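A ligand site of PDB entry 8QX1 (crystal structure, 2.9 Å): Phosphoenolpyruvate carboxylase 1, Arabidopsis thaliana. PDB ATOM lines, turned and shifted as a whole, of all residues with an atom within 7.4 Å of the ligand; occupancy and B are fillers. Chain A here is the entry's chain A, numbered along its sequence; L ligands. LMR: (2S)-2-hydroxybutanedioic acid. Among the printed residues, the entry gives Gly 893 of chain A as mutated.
An oxygen (O2) of the ligand is in hydrogen-bond range of the side-chain amide oxygen of Asn 972 (2.6 Å).
An oxygen (O4B) of the ligand lies within salt-bridge range of the guanidinium group of Arg 897 (2.6 Å).
The side-chain amino group (NZ) of Lys 838 lies within salt-bridge range of an oxygen (O4A) of the ligand, 2.9 Å away.
The guanidinium group (NE) of Arg 650 lies within salt-bridge range of an oxygen (O1A) of the ligand, 2.9 Å away.
An oxygen (O2) of the ligand sits at hydrogen-bond distance from the backbone NH (N) of Gly 651.
O of Asn 972 sits at hydrogen-bond distance from NZ of Lys 838 (2.8 Å).
NH2 of Arg 897 is in salt-bridge range of OE1 of Glu 116, 3.1 Å away.
The guanidinium group (NH1) of Arg 897 is in hydrogen-bond range of the backbone carbonyl oxygen (O) of Gly 969 (2.9 Å).
The guanidinium group of Arg 897 lies within hydrogen-bond range of the side-chain amide oxygen of Asn 113, 3.2 Å away.
The side-chain amino group (NZ) of Lys 838 is in hydrogen-bond range of the side-chain sulfur (SD) of Met 834 (3.6 Å).
The backbone carbonyl oxygen (O) of Leu 970 sits at hydrogen-bond distance from the side-chain amino group (NZ) of Lys 838 (2.5 Å).
The side-chain amide oxygen of Gln 971 lies close to the side-chain amide oxygen of Gln 682 (3.3 Å).
The side-chain amide oxygen of Gln 971 sits close to the backbone carbonyl oxygen of Glu 678 (3.2 Å).
Pro 654 touches the ligand (CG to O1B, 3.9 Å).
Gln 682 touches the ligand.
Met 834 touches the ligand.
Leu 890 touches the ligand (CD2 to O1B, 3.5 Å).
O of Leu 970 touches O4A of the ligand, 3.9 Å away.
Gln 971 touches the ligand.
Hydrophobic or aromatic side chains within 4 Å of the ligand: Pro 654, Met 834 and Leu 890.
Within 4 Å of the ligand: Arg 650, Gly 651, Pro 654, Gln 682, Met 834, Lys 838, Leu 890, Arg 897, Leu 970, Gln 971 and Asn 972.
The nearest printed residue that does not touch the ligand is Leu 894 (4.3 Å).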
ATOM      1  N   ASN A 113      16.609  36.912 -26.835  1.00  0.00           N
ATOM      2  CA  ASN A 113      16.638  35.503 -27.197  1.00  0.00           C
ATOM      3  C   ASN A 113      15.654  35.200 -28.320  1.00  0.00           C
ATOM      4  O   ASN A 113      15.991  34.477 -29.263  1.00  0.00           O
ATOM      5  CB  ASN A 113      16.332  34.619 -25.985  1.00  0.00           C
ATOM      6  CG  ASN A 113      17.474  34.573 -24.983  1.00  0.00           C
ATOM      7  OD1 ASN A 113      18.644  34.672 -25.350  1.00  0.00           O
ATOM      8  ND2 ASN A 113      17.130  34.400 -23.707  1.00  0.00           N
ATOM      9  N   GLU A 116      16.959  36.328 -31.539  1.00  0.00           N
ATOM     10  CA  GLU A 116      18.030  35.461 -31.994  1.00  0.00           C
ATOM     11  C   GLU A 116      17.493  34.157 -32.585  1.00  0.00           C
ATOM     12  O   GLU A 116      17.981  33.685 -33.624  1.00  0.00           O
ATOM     13  CB  GLU A 116      19.005  35.161 -30.858  1.00  0.00           C
ATOM     14  CG  GLU A 116      20.274  34.479 -31.346  1.00  0.00           C
ATOM     15  CD  GLU A 116      21.105  33.892 -30.233  1.00  0.00           C
ATOM     16  OE1 GLU A 116      21.079  34.445 -29.111  1.00  0.00           O
ATOM     17  OE2 GLU A 116      21.778  32.861 -30.471  1.00  0.00           O
ATOM     18  N   ILE A 120      17.969  32.800 -36.382  1.00  0.00           N
ATOM     19  CA  ILE A 120      18.508  31.478 -36.681  1.00  0.00           C
ATOM     20  C   ILE A 120      17.577  30.716 -37.605  1.00  0.00           C
ATOM     21  O   ILE A 120      18.011  30.051 -38.549  1.00  0.00           O
ATOM     22  CB  ILE A 120      18.744  30.696 -35.368  1.00  0.00           C
ATOM     23  CG1 ILE A 120      19.972  31.250 -34.640  1.00  0.00           C
ATOM     24  CG2 ILE A 120      18.896  29.222 -35.668  1.00  0.00           C
ATOM     25  CD1 ILE A 120      20.041  30.856 -33.182  1.00  0.00           C
ATOM     26  N   SER A 138      30.205  22.278 -37.286  1.00  0.00           N
ATOM     27  CA  SER A 138      30.145  22.890 -35.963  1.00  0.00           C
ATOM     28  C   SER A 138      29.228  24.110 -35.919  1.00  0.00           C
ATOM     29  O   SER A 138      29.095  24.717 -34.854  1.00  0.00           O
ATOM     30  CB  SER A 138      31.547  23.265 -35.488  1.00  0.00           C
ATOM     31  OG  SER A 138      32.211  24.018 -36.482  1.00  0.00           O
ATOM     32  N   THR A 647      29.423  17.868 -24.650  1.00  0.00           N
ATOM     33  CA  THR A 647      29.475  18.557 -25.936  1.00  0.00           C
ATOM     34  C   THR A 647      28.230  18.285 -26.747  1.00  0.00           C
ATOM     35  O   THR A 647      27.791  19.138 -27.529  1.00  0.00           O
ATOM     36  CB  THR A 647      30.714  18.126 -26.737  1.00  0.00           C
ATOM     37  OG1 THR A 647      31.054  16.774 -26.376  1.00  0.00           O
ATOM     38  CG2 THR A 647      31.878  19.050 -26.471  1.00  0.00           C
ATOM     39  N   GLY A 649      25.338  18.068 -25.587  1.00  0.00           N
ATOM     40  CA  GLY A 649      24.249  18.789 -24.951  1.00  0.00           C
ATOM     41  C   GLY A 649      24.185  20.265 -25.285  1.00  0.00           C
ATOM     42  O   GLY A 649      23.384  20.986 -24.665  1.00  0.00           O
ATOM     43  N   ARG A 650      25.000  20.738 -26.223  1.00  0.00           N
ATOM     44  CA  ARG A 650      25.015  22.145 -26.621  1.00  0.00           C
ATOM     45  C   ARG A 650      23.805  22.463 -27.510  1.00  0.00           C
ATOM     46  O   ARG A 650      22.995  21.596 -27.845  1.00  0.00           O
ATOM     47  CB  ARG A 650      26.319  22.479 -27.347  1.00  0.00           C
ATOM     48  CG  ARG A 650      27.583  22.434 -26.480  1.00  0.00           C
ATOM     49  CD  ARG A 650      28.813  22.976 -27.221  1.00  0.00           C
ATOM     50  NE  ARG A 650      28.660  24.380 -27.601  1.00  0.00           N
ATOM     51  CZ  ARG A 650      29.554  25.078 -28.297  1.00  0.00           C
ATOM     52  NH1 ARG A 650      30.688  24.509 -28.690  1.00  0.00           N
ATOM     53  NH2 ARG A 650      29.326  26.348 -28.596  1.00  0.00           N
ATOM     54  N   GLY A 651      23.686  23.728 -27.884  1.00  0.00           N
ATOM     55  CA  GLY A 651      22.590  24.127 -28.742  1.00  0.00           C
ATOM     56  C   GLY A 651      23.010  24.376 -30.174  1.00  0.00           C
ATOM     57  O   GLY A 651      23.883  25.201 -30.443  1.00  0.00           O
ATOM     58  N   GLY A 652      22.393  23.658 -31.113  1.00  0.00           N
ATOM     59  CA  GLY A 652      22.575  23.956 -32.512  1.00  0.00           C
ATOM     60  C   GLY A 652      23.678  23.171 -33.199  1.00  0.00           C
ATOM     61  O   GLY A 652      23.890  21.992 -32.905  1.00  0.00           O
ATOM     62  N   GLY A 653      24.388  23.847 -34.108  1.00  0.00           N
ATOM     63  CA  GLY A 653      25.421  23.189 -34.893  1.00  0.00           C
ATOM     64  C   GLY A 653      26.467  22.424 -34.115  1.00  0.00           C
ATOM     65  O   GLY A 653      26.856  21.326 -34.536  1.00  0.00           O
ATOM     66  N   PRO A 654      26.981  22.954 -33.002  1.00  0.00           N
ATOM     67  CA  PRO A 654      27.995  22.210 -32.236  1.00  0.00           C
ATOM     68  C   PRO A 654      27.622  20.766 -31.961  1.00  0.00           C
ATOM     69  O   PRO A 654      28.514  19.898 -31.942  1.00  0.00           O
ATOM     70  CB  PRO A 654      28.076  23.018 -30.932  1.00  0.00           C
ATOM     71  CG  PRO A 654      27.887  24.399 -31.391  1.00  0.00           C
ATOM     72  CD  PRO A 654      26.908  24.351 -32.535  1.00  0.00           C
ATOM     73  N   THR A 655      26.333  20.475 -31.769  1.00  0.00           N
ATOM     74  CA  THR A 655      25.924  19.100 -31.481  1.00  0.00           C
ATOM     75  C   THR A 655      26.281  18.161 -32.620  1.00  0.00           C
ATOM     76  O   THR A 655      26.623  16.999 -32.387  1.00  0.00           O
ATOM     77  CB  THR A 655      24.421  19.053 -31.191  1.00  0.00           C
ATOM     78  OG1 THR A 655      24.111  19.978 -30.142  1.00  0.00           O
ATOM     79  CG2 THR A 655      23.995  17.672 -30.760  1.00  0.00           C
ATOM     80  N   GLU A 678      17.916  24.124 -20.136  1.00  0.00           N
ATOM     81  CA  GLU A 678      18.389  25.453 -20.546  1.00  0.00           C
ATOM     82  C   GLU A 678      18.565  25.583 -22.050  1.00  0.00           C
ATOM     83  O   GLU A 678      18.965  26.666 -22.511  1.00  0.00           O
ATOM     84  CB  GLU A 678      19.710  25.776 -19.826  1.00  0.00           C
ATOM     85  CG  GLU A 678      20.692  24.594 -19.742  1.00  0.00           C
ATOM     86  CD  GLU A 678      20.678  23.891 -18.382  1.00  0.00           C
ATOM     87  OE1 GLU A 678      21.141  24.503 -17.397  1.00  0.00           O
ATOM     88  OE2 GLU A 678      20.213  22.744 -18.305  1.00  0.00           O
ATOM     89  N   VAL A 679      18.280  24.542 -22.827  1.00  0.00           N
ATOM     90  CA  VAL A 679      18.494  24.553 -24.263  1.00  0.00           C
ATOM     91  C   VAL A 679      17.218  24.134 -25.000  1.00  0.00           C
ATOM     92  O   VAL A 679      17.092  24.320 -26.206  1.00  0.00           O
ATOM     93  CB  VAL A 679      19.676  23.651 -24.642  1.00  0.00           C
ATOM     94  CG1 VAL A 679      20.110  23.880 -26.079  1.00  0.00           C
ATOM     95  CG2 VAL A 679      20.836  23.878 -23.702  1.00  0.00           C
ATOM     96  N   GLN A 682      15.444  26.765 -27.207  1.00  0.00           N
ATOM     97  CA  GLN A 682      16.225  27.057 -28.402  1.00  0.00           C
ATOM     98  C   GLN A 682      16.155  25.928 -29.423  1.00  0.00           C
ATOM     99  O   GLN A 682      16.325  26.157 -30.628  1.00  0.00           O
ATOM    100  CB  GLN A 682      17.679  27.333 -28.006  1.00  0.00           C
ATOM    101  CG  GLN A 682      18.674  27.505 -29.148  1.00  0.00           C
ATOM    102  CD  GLN A 682      20.132  27.508 -28.684  1.00  0.00           C
ATOM    103  OE1 GLN A 682      20.419  27.248 -27.508  1.00  0.00           O
ATOM    104  NE2 GLN A 682      21.044  27.816 -29.595  1.00  0.00           N
ATOM    105  N   LEU A 831      33.913  24.139 -26.679  1.00  0.00           N
ATOM    106  CA  LEU A 831      33.030  24.403 -25.542  1.00  0.00           C
ATOM    107  C   LEU A 831      33.658  25.382 -24.561  1.00  0.00           C
ATOM    108  O   LEU A 831      33.009  26.321 -24.095  1.00  0.00           O
ATOM    109  CB  LEU A 831      32.667  23.092 -24.853  1.00  0.00           C
ATOM    110  CG  LEU A 831      31.422  23.068 -23.964  1.00  0.00           C
ATOM    111  CD1 LEU A 831      30.863  21.661 -23.900  1.00  0.00           C
ATOM    112  CD2 LEU A 831      31.750  23.572 -22.574  1.00  0.00           C
ATOM    113  N   MET A 834      33.548  28.898 -25.966  1.00  0.00           N
ATOM    114  CA  MET A 834      32.207  29.449 -25.855  1.00  0.00           C
ATOM    115  C   MET A 834      31.906  29.888 -24.428  1.00  0.00           C
ATOM    116  O   MET A 834      31.293  30.942 -24.218  1.00  0.00           O
ATOM    117  CB  MET A 834      31.176  28.428 -26.323  1.00  0.00           C
ATOM    118  CG  MET A 834      29.732  28.900 -26.199  1.00  0.00           C
ATOM    119  SD  MET A 834      28.959  28.474 -24.630  1.00  0.00           S
ATOM    120  CE  MET A 834      28.738  26.721 -24.847  1.00  0.00           C
ATOM    121  N   LYS A 838      31.030  33.888 -22.543  1.00  0.00           N
ATOM    122  CA  LYS A 838      30.038  34.280 -21.535  1.00  0.00           C
ATOM    123  C   LYS A 838      30.679  34.714 -20.219  1.00  0.00           C
ATOM    124  O   LYS A 838      29.950  35.019 -19.275  1.00  0.00           O
ATOM    125  CB  LYS A 838      29.067  33.129 -21.281  1.00  0.00           C
ATOM    126  CG  LYS A 838      28.418  32.593 -22.545  1.00  0.00           C
ATOM    127  CD  LYS A 838      27.575  31.385 -22.228  1.00  0.00           C
ATOM    128  CE  LYS A 838      26.693  31.022 -23.399  1.00  0.00           C
ATOM    129  NZ  LYS A 838      25.942  29.771 -23.105  1.00  0.00           N
ATOM    130  N   ASP A 887      32.939  31.332 -35.442  1.00  0.00           N
ATOM    131  CA  ASP A 887      31.475  31.305 -35.404  1.00  0.00           C
ATOM    132  C   ASP A 887      30.970  32.711 -35.086  1.00  0.00           C
ATOM    133  O   ASP A 887      30.508  32.989 -33.974  1.00  0.00           O
ATOM    134  CB  ASP A 887      30.977  30.275 -34.392  1.00  0.00           C
ATOM    135  CG  ASP A 887      29.514  29.927 -34.573  1.00  0.00           C
ATOM    136  OD1 ASP A 887      28.835  30.587 -35.395  1.00  0.00           O
ATOM    137  OD2 ASP A 887      29.042  28.986 -33.900  1.00  0.00           O
ATOM    138  N   LEU A 890      27.256  33.274 -33.601  1.00  0.00           N
ATOM    139  CA  LEU A 890      27.095  33.008 -32.170  1.00  0.00           C
ATOM    140  C   LEU A 890      27.771  34.080 -31.334  1.00  0.00           C
ATOM    141  O   LEU A 890      27.202  34.556 -30.338  1.00  0.00           O
ATOM    142  CB  LEU A 890      27.638  31.616 -31.832  1.00  0.00           C
ATOM    143  CG  LEU A 890      27.767  31.185 -30.364  1.00  0.00           C
ATOM    144  CD1 LEU A 890      26.474  31.358 -29.586  1.00  0.00           C
ATOM    145  CD2 LEU A 890      28.185  29.738 -30.325  1.00  0.00           C
ATOM    146  N   GLY A 893      25.371  36.956 -31.247  1.00  0.00           N
ATOM    147  CA  GLY A 893      24.202  36.782 -30.381  1.00  0.00           C
ATOM    148  C   GLY A 893      24.543  36.843 -28.898  1.00  0.00           C
ATOM    149  O   GLY A 893      23.821  37.452 -28.107  1.00  0.00           O
ATOM    150  N   LEU A 894      25.667  36.220 -28.515  1.00  0.00           N
ATOM    151  CA  LEU A 894      26.098  36.276 -27.122  1.00  0.00           C
ATOM    152  C   LEU A 894      26.451  37.709 -26.723  1.00  0.00           C
ATOM    153  O   LEU A 894      26.084  38.153 -25.627  1.00  0.00           O
ATOM    154  CB  LEU A 894      27.296  35.344 -26.898  1.00  0.00           C
ATOM    155  CG  LEU A 894      27.087  33.827 -27.050  1.00  0.00           C
ATOM    156  CD1 LEU A 894      28.369  33.063 -26.700  1.00  0.00           C
ATOM    157  CD2 LEU A 894      25.932  33.329 -26.200  1.00  0.00           C
ATOM    158  N   ARG A 897      23.199  39.476 -25.907  1.00  0.00           N
ATOM    159  CA  ARG A 897      22.644  39.184 -24.589  1.00  0.00           C
ATOM    160  C   ARG A 897      23.463  39.832 -23.472  1.00  0.00           C
ATOM    161  O   ARG A 897      22.905  40.277 -22.458  1.00  0.00           O
ATOM    162  CB  ARG A 897      22.554  37.686 -24.345  1.00  0.00           C
ATOM    163  CG  ARG A 897      21.737  36.916 -25.331  1.00  0.00           C
ATOM    164  CD  ARG A 897      21.700  35.485 -24.873  1.00  0.00           C
ATOM    165  NE  ARG A 897      21.742  34.536 -25.970  1.00  0.00           N
ATOM    166  CZ  ARG A 897      22.194  33.300 -25.866  1.00  0.00           C
ATOM    167  NH1 ARG A 897      22.672  32.867 -24.700  1.00  0.00           N
ATOM    168  NH2 ARG A 897      22.202  32.500 -26.918  1.00  0.00           N
ATOM    169  N   ALA A 968      18.716  32.623 -17.696  1.00  0.00           N
ATOM    170  CA  ALA A 968      18.151  32.576 -19.042  1.00  0.00           C
ATOM    171  C   ALA A 968      19.094  33.174 -20.087  1.00  0.00           C
ATOM    172  O   ALA A 968      19.028  32.797 -21.266  1.00  0.00           O
ATOM    173  CB  ALA A 968      16.800  33.290 -19.070  1.00  0.00           C
ATOM    174  N   GLY A 969      19.965  34.096 -19.691  1.00  0.00           N
ATOM    175  CA  GLY A 969      20.868  34.692 -20.663  1.00  0.00           C
ATOM    176  C   GLY A 969      22.137  33.908 -20.908  1.00  0.00           C
ATOM    177  O   GLY A 969      22.724  33.987 -21.992  1.00  0.00           O
ATOM    178  N   LEU A 970      22.601  33.162 -19.904  1.00  0.00           N
ATOM    179  CA  LEU A 970      23.793  32.366 -20.127  1.00  0.00           C
ATOM    180  C   LEU A 970      23.490  30.963 -20.611  1.00  0.00           C
ATOM    181  O   LEU A 970      24.378  30.315 -21.175  1.00  0.00           O
ATOM    182  CB  LEU A 970      24.624  32.312 -18.843  1.00  0.00           C
ATOM    183  CG  LEU A 970      25.007  33.726 -18.391  1.00  0.00           C
ATOM    184  CD1 LEU A 970      25.884  33.669 -17.177  1.00  0.00           C
ATOM    185  CD2 LEU A 970      25.702  34.453 -19.519  1.00  0.00           C
ATOM    186  N   GLN A 971      22.250  30.503 -20.436  1.00  0.00           N
ATOM    187  CA  GLN A 971      21.803  29.187 -20.886  1.00  0.00           C
ATOM    188  C   GLN A 971      22.806  28.109 -20.466  1.00  0.00           C
ATOM    189  O   GLN A 971      23.146  28.040 -19.280  1.00  0.00           O
ATOM    190  CB  GLN A 971      21.578  29.197 -22.398  1.00  0.00           C
ATOM    191  CG  GLN A 971      20.434  30.148 -22.777  1.00  0.00           C
ATOM    192  CD  GLN A 971      19.909  29.963 -24.199  1.00  0.00           C
ATOM    193  OE1 GLN A 971      19.760  28.842 -24.699  1.00  0.00           O
ATOM    194  NE2 GLN A 971      19.584  31.081 -24.839  1.00  0.00           N
ATOM    195  N   ASN A 972      23.292  27.309 -21.410  1.00  0.00           N
ATOM    196  CA  ASN A 972      24.140  26.165 -21.086  1.00  0.00           C
ATOM    197  C   ASN A 972      25.621  26.543 -21.081  1.00  0.00           C
ATOM    198  O   ASN A 972      26.098  27.253 -21.963  1.00  0.00           O
ATOM    199  CB  ASN A 972      23.902  25.020 -22.076  1.00  0.00           C
ATOM    200  CG  ASN A 972      24.312  25.379 -23.494  1.00  0.00           C
ATOM    201  OD1 ASN A 972      23.612  26.118 -24.186  1.00  0.00           O
ATOM    202  ND2 ASN A 972      25.448  24.859 -23.946  1.00  0.00           N
ATOM    203  N   THR A 973      26.345  26.037 -20.079  1.00  0.00           N
ATOM    204  CA  THR A 973      27.794  26.187 -20.033  1.00  0.00           C
ATOM    205  C   THR A 973      28.468  24.826 -19.873  1.00  0.00           C
ATOM    206  O   THR A 973      28.981  24.256 -20.840  1.00  0.00           O
ATOM    207  CB  THR A 973      28.225  27.128 -18.902  1.00  0.00           C
ATOM    208  OG1 THR A 973      27.626  26.714 -17.673  1.00  0.00           O
ATOM    209  CG2 THR A 973      27.794  28.545 -19.202  1.00  0.00           C
HETATM  210  C1  LMR L   1      25.830  26.756 -27.867  1.00  0.00           C
HETATM  211  O1A LMR L   1      26.183  25.816 -27.097  1.00  0.00           O
HETATM  212  O1B LMR L   1      26.475  27.008 -28.917  1.00  0.00           O
HETATM  213  C2  LMR L   1      24.639  27.560 -27.530  1.00  0.00           C
HETATM  214  O2  LMR L   1      23.781  26.787 -26.648  1.00  0.00           O
HETATM  215  C3  LMR L   1      25.089  28.867 -26.859  1.00  0.00           C
HETATM  216  C4  LMR L   1      23.873  29.597 -26.300  1.00  0.00           C
HETATM  217  O4A LMR L   1      23.778  29.800 -25.037  1.00  0.00           O
HETATM  218  O4B LMR L   1      22.975  30.002 -27.085  1.00  0.00           O
